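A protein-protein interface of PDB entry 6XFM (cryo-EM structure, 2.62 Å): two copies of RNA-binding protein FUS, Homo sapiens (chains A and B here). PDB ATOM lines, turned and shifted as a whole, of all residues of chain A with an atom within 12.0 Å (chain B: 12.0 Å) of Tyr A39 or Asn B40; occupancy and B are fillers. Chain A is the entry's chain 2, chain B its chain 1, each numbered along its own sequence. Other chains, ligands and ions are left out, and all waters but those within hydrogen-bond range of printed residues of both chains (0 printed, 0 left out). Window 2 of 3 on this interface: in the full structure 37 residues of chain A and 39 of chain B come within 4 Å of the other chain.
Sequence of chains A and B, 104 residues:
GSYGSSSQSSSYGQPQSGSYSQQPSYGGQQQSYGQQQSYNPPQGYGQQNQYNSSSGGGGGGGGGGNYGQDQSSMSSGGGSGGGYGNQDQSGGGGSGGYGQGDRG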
ATOM      1  N   SER A   2      16.996 -12.561  -6.418  1.00  0.00           N
ATOM      2  CA  SER A   2      16.828 -11.632  -5.265  1.00  0.00           C
ATOM      3  C   SER A   2      17.492 -10.296  -5.587  1.00  0.00           C
ATOM      4  O   SER A   2      18.388  -9.841  -4.868  1.00  0.00           O
ATOM      5  CB  SER A   2      17.471 -12.251  -4.024  1.00  0.00           C
ATOM      6  OG  SER A   2      18.596 -13.024  -4.420  1.00  0.00           O
ATOM      7  N   GLN A  35      16.429  -1.457  -6.407  1.00  0.00           N
ATOM      8  CA  GLN A  35      16.779  -1.917  -5.072  1.00  0.00           C
ATOM      9  C   GLN A  35      16.072  -3.200  -4.652  1.00  0.00           C
ATOM     10  O   GLN A  35      15.034  -3.590  -5.192  1.00  0.00           O
ATOM     11  CB  GLN A  35      16.455  -0.809  -4.070  1.00  0.00           C
ATOM     12  CG  GLN A  35      14.963  -0.469  -4.143  1.00  0.00           C
ATOM     13  CD  GLN A  35      14.695   0.846  -3.422  1.00  0.00           C
ATOM     14  OE1 GLN A  35      15.166   1.897  -3.855  1.00  0.00           O
ATOM     15  NE2 GLN A  35      13.961   0.852  -2.345  1.00  0.00           N
ATOM     16  N   GLN A  36      16.663  -3.831  -3.645  1.00  0.00           N
ATOM     17  CA  GLN A  36      16.132  -5.060  -3.074  1.00  0.00           C
ATOM     18  C   GLN A  36      15.924  -4.843  -1.579  1.00  0.00           C
ATOM     19  O   GLN A  36      16.834  -4.384  -0.889  1.00  0.00           O
ATOM     20  CB  GLN A  36      17.120  -6.206  -3.308  1.00  0.00           C
ATOM     21  CG  GLN A  36      16.426  -7.551  -3.072  1.00  0.00           C
ATOM     22  CD  GLN A  36      16.462  -7.912  -1.589  1.00  0.00           C
ATOM     23  OE1 GLN A  36      15.449  -8.326  -1.027  1.00  0.00           O
ATOM     24  NE2 GLN A  36      17.577  -7.788  -0.921  1.00  0.00           N
ATOM     25  N   GLN A  37      14.724  -5.132  -1.083  1.00  0.00           N
ATOM     26  CA  GLN A  37      14.437  -4.913   0.334  1.00  0.00           C
ATOM     27  C   GLN A  37      13.892  -6.169   1.003  1.00  0.00           C
ATOM     28  O   GLN A  37      13.105  -6.908   0.412  1.00  0.00           O
ATOM     29  CB  GLN A  37      13.410  -3.789   0.472  1.00  0.00           C
ATOM     30  CG  GLN A  37      14.043  -2.470   0.037  1.00  0.00           C
ATOM     31  CD  GLN A  37      12.974  -1.387  -0.047  1.00  0.00           C
ATOM     32  OE1 GLN A  37      11.812  -1.682  -0.321  1.00  0.00           O
ATOM     33  NE2 GLN A  37      13.301  -0.144   0.172  1.00  0.00           N
ATOM     34  N   SER A  38      14.303  -6.389   2.252  1.00  0.00           N
ATOM     35  CA  SER A  38      13.835  -7.545   3.004  1.00  0.00           C
ATOM     36  C   SER A  38      13.568  -7.154   4.457  1.00  0.00           C
ATOM     37  O   SER A  38      14.296  -6.344   5.039  1.00  0.00           O
ATOM     38  CB  SER A  38      14.888  -8.655   2.960  1.00  0.00           C
ATOM     39  OG  SER A  38      16.077  -8.198   3.591  1.00  0.00           O
ATOM     40  N   TYR A  39      12.527  -7.743   5.039  1.00  0.00           N
ATOM     41  CA  TYR A  39      12.176  -7.454   6.424  1.00  0.00           C
ATOM     42  C   TYR A  39      12.224  -8.729   7.260  1.00  0.00           C
ATOM     43  O   TYR A  39      11.522  -9.697   6.969  1.00  0.00           O
ATOM     44  CB  TYR A  39      10.770  -6.852   6.488  1.00  0.00           C
ATOM     45  CG  TYR A  39      10.427  -6.517   7.920  1.00  0.00           C
ATOM     46  CD1 TYR A  39      10.839  -5.297   8.468  1.00  0.00           C
ATOM     47  CD2 TYR A  39       9.702  -7.427   8.698  1.00  0.00           C
ATOM     48  CE1 TYR A  39      10.523  -4.985   9.795  1.00  0.00           C
ATOM     49  CE2 TYR A  39       9.386  -7.114  10.027  1.00  0.00           C
ATOM     50  CZ  TYR A  39       9.798  -5.894  10.576  1.00  0.00           C
ATOM     51  OH  TYR A  39       9.490  -5.587  11.884  1.00  0.00           O
ATOM     52  N   ASN A  40      13.056  -8.727   8.296  1.00  0.00           N
ATOM     53  CA  ASN A  40      13.185  -9.893   9.162  1.00  0.00           C
ATOM     54  C   ASN A  40      13.556 -11.126   8.344  1.00  0.00           C
ATOM     55  O   ASN A  40      14.707 -11.229   7.951  1.00  0.00           O
ATOM     56  CB  ASN A  40      11.869 -10.144   9.901  1.00  0.00           C
ATOM     57  CG  ASN A  40      12.052 -11.249  10.936  1.00  0.00           C
ATOM     58  OD1 ASN A  40      13.033 -11.993  10.887  1.00  0.00           O
ATOM     59  ND2 ASN A  40      11.160 -11.403  11.876  1.00  0.00           N
ATOM     60  N   GLN B  35      12.420  -3.360  -8.487  1.00  0.00           N
ATOM     61  CA  GLN B  35      12.795  -3.857  -7.172  1.00  0.00           C
ATOM     62  C   GLN B  35      12.116  -5.162  -6.792  1.00  0.00           C
ATOM     63  O   GLN B  35      11.078  -5.540  -7.335  1.00  0.00           O
ATOM     64  CB  GLN B  35      12.459  -2.791  -6.132  1.00  0.00           C
ATOM     65  CG  GLN B  35      10.961  -2.478  -6.179  1.00  0.00           C
ATOM     66  CD  GLN B  35      10.673  -1.196  -5.410  1.00  0.00           C
ATOM     67  OE1 GLN B  35      11.123  -0.122  -5.807  1.00  0.00           O
ATOM     68  NE2 GLN B  35       9.946  -1.243  -4.328  1.00  0.00           N
ATOM     69  N   GLN B  36      12.725  -5.822  -5.814  1.00  0.00           N
ATOM     70  CA  GLN B  36      12.220  -7.080  -5.282  1.00  0.00           C
ATOM     71  C   GLN B  36      12.023  -6.918  -3.778  1.00  0.00           C
ATOM     72  O   GLN B  36      12.931  -6.468  -3.081  1.00  0.00           O
ATOM     73  CB  GLN B  36      13.223  -8.200  -5.565  1.00  0.00           C
ATOM     74  CG  GLN B  36      12.555  -9.563  -5.369  1.00  0.00           C
ATOM     75  CD  GLN B  36      12.614  -9.978  -3.901  1.00  0.00           C
ATOM     76  OE1 GLN B  36      11.614 -10.429  -3.343  1.00  0.00           O
ATOM     77  NE2 GLN B  36      13.733  -9.858  -3.240  1.00  0.00           N
ATOM     78  N   GLN B  37      10.834  -7.248  -3.280  1.00  0.00           N
ATOM     79  CA  GLN B  37      10.556  -7.084  -1.853  1.00  0.00           C
ATOM     80  C   GLN B  37      10.042  -8.373  -1.224  1.00  0.00           C
ATOM     81  O   GLN B  37       9.265  -9.108  -1.832  1.00  0.00           O
ATOM     82  CB  GLN B  37       9.509  -5.986  -1.668  1.00  0.00           C
ATOM     83  CG  GLN B  37      10.112  -4.640  -2.062  1.00  0.00           C
ATOM     84  CD  GLN B  37       9.023  -3.575  -2.097  1.00  0.00           C
ATOM     85  OE1 GLN B  37       7.864  -3.881  -2.372  1.00  0.00           O
ATOM     86  NE2 GLN B  37       9.329  -2.335  -1.835  1.00  0.00           N
ATOM     87  N   SER B  38      10.467  -8.626   0.013  1.00  0.00           N
ATOM     88  CA  SER B  38      10.029  -9.816   0.730  1.00  0.00           C
ATOM     89  C   SER B  38       9.769  -9.479   2.198  1.00  0.00           C
ATOM     90  O   SER B  38      10.484  -8.671   2.799  1.00  0.00           O
ATOM     91  CB  SER B  38      11.102 -10.904   0.637  1.00  0.00           C
ATOM     92  OG  SER B  38      12.288 -10.448   1.273  1.00  0.00           O
ATOM     93  N   TYR B  39       8.749 -10.111   2.772  1.00  0.00           N
ATOM     94  CA  TYR B  39       8.405  -9.874   4.168  1.00  0.00           C
ATOM     95  C   TYR B  39       8.485 -11.175   4.959  1.00  0.00           C
ATOM     96  O   TYR B  39       7.797 -12.146   4.643  1.00  0.00           O
ATOM     97  CB  TYR B  39       6.987  -9.301   4.264  1.00  0.00           C
ATOM     98  CG  TYR B  39       6.651  -9.022   5.709  1.00  0.00           C
ATOM     99  CD1 TYR B  39       7.043  -7.814   6.296  1.00  0.00           C
ATOM    100  CD2 TYR B  39       5.950  -9.971   6.463  1.00  0.00           C
ATOM    101  CE1 TYR B  39       6.734  -7.554   7.637  1.00  0.00           C
ATOM    102  CE2 TYR B  39       5.640  -9.711   7.804  1.00  0.00           C
ATOM    103  CZ  TYR B  39       6.032  -8.501   8.391  1.00  0.00           C
ATOM    104  OH  TYR B  39       5.730  -8.245   9.712  1.00  0.00           O
ATOM    105  N   ASN B  40       9.327 -11.192   5.985  1.00  0.00           N
ATOM    106  CA  ASN B  40       9.485 -12.386   6.806  1.00  0.00           C
ATOM    107  C   ASN B  40       9.868 -13.583   5.940  1.00  0.00           C
ATOM    108  O   ASN B  40      11.015 -13.653   5.531  1.00  0.00           O
ATOM    109  CB  ASN B  40       8.183 -12.686   7.549  1.00  0.00           C
ATOM    110  CG  ASN B  40       8.397 -13.822   8.544  1.00  0.00           C
ATOM    111  OD1 ASN B  40       9.393 -14.543   8.460  1.00  0.00           O
ATOM    112  ND2 ASN B  40       7.517 -14.027   9.486  1.00  0.00           N
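O of Ser B38 lies within hydrogen-bond range of N of Tyr A39, 3.2 Å away. The backbone carbonyl oxygen of Gln A37 lies within hydrogen-bond range of the backbone NH of Ser B38, at 3.2 Å. N of Gln B36 lies within hydrogen-bond range of O of Gln A35 (3.3 Å). The backbone carbonyl oxygen of Gln B36 is in hydrogen-bond range of the backbone NH of Gln A37. The backbone carbonyl oxygen (O) of Tyr A39 lies within hydrogen-bond range of the backbone NH (N) of Asn B40 (2.8 Å). The side-chain amide nitrogen of Gln B37 sits at hydrogen-bond distance from the side-chain amide oxygen of Gln A37 (3.0 Å). The side-chain amide nitrogen of Gln B36 sits at hydrogen-bond distance from the side-chain amide oxygen of Gln A36 (3.2 Å).
NE2 of Gln B35 lies close to NE2 of Gln B37 (2.8 Å). NE2 of Gln A37 lies close to NE2 of Gln A35.
Among the printed residues, merely in contact across the chains: Gln A35 with Gln B35 (2.9 Å), Ser A38 with Ser B38 (3.5 Å) and Tyr A39 with Tyr B39 (3.2 Å).
Ser A2 touches none of the printed residues of chain B. Of the printed residues of chain B, Gln A35 touches Gln B35 (2.9 Å) and Gln B36 (3.3 Å). Printed residues of chain B within 4 Å of Gln A36: Gln B36 (3.2 Å). Of chain B, only Ser B38 comes within 4 Å of Ser A38. Of chain B, only Ser B38, Tyr B39 and Asn B40 come within 4 Å of Tyr A39. No residue of chain B comes within 4 Å of Asn A40. Printed residues of chain A within 4 Å of Gln B35: Gln A35. Of the printed residues of chain A, Gln B36 touches Gln A35, Gln A36 and Gln A37. Of the printed residues of chain A, Gln B37 touches Gln A37. Tyr B39 touches just one residue of chain A: Tyr A39. Of chain A, only Tyr A39 comes within 4 Å of Asn B40. The nearest residue of chain B that does not touch Tyr A39 is Gln B37 (6.8 Å).
Of the 6 printed residues of chain B, 6 touch a printed residue of chain A. Printed residues of chain B that touch a printed residue of chain A: Gln B35, Gln B36, Gln B37, Ser B38, Tyr B39 and Asn B40. Among the printed residues, 10 pairs touch across the chains.
Gln A35 touches its own counterpart, Gln B35. Gln A35 touches Gln B36, but with the chains exchanged Gln A36 does not touch Gln B35 (5.0 Å). Gln A37 touches Gln B36, but with the chains exchanged Gln A36 does not touch Gln B37 (5.1 Å). Tyr B39 touches its own counterpart, Tyr A39. Positions printed for both chains: 35, 36, 37, 38, 39 and 40.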
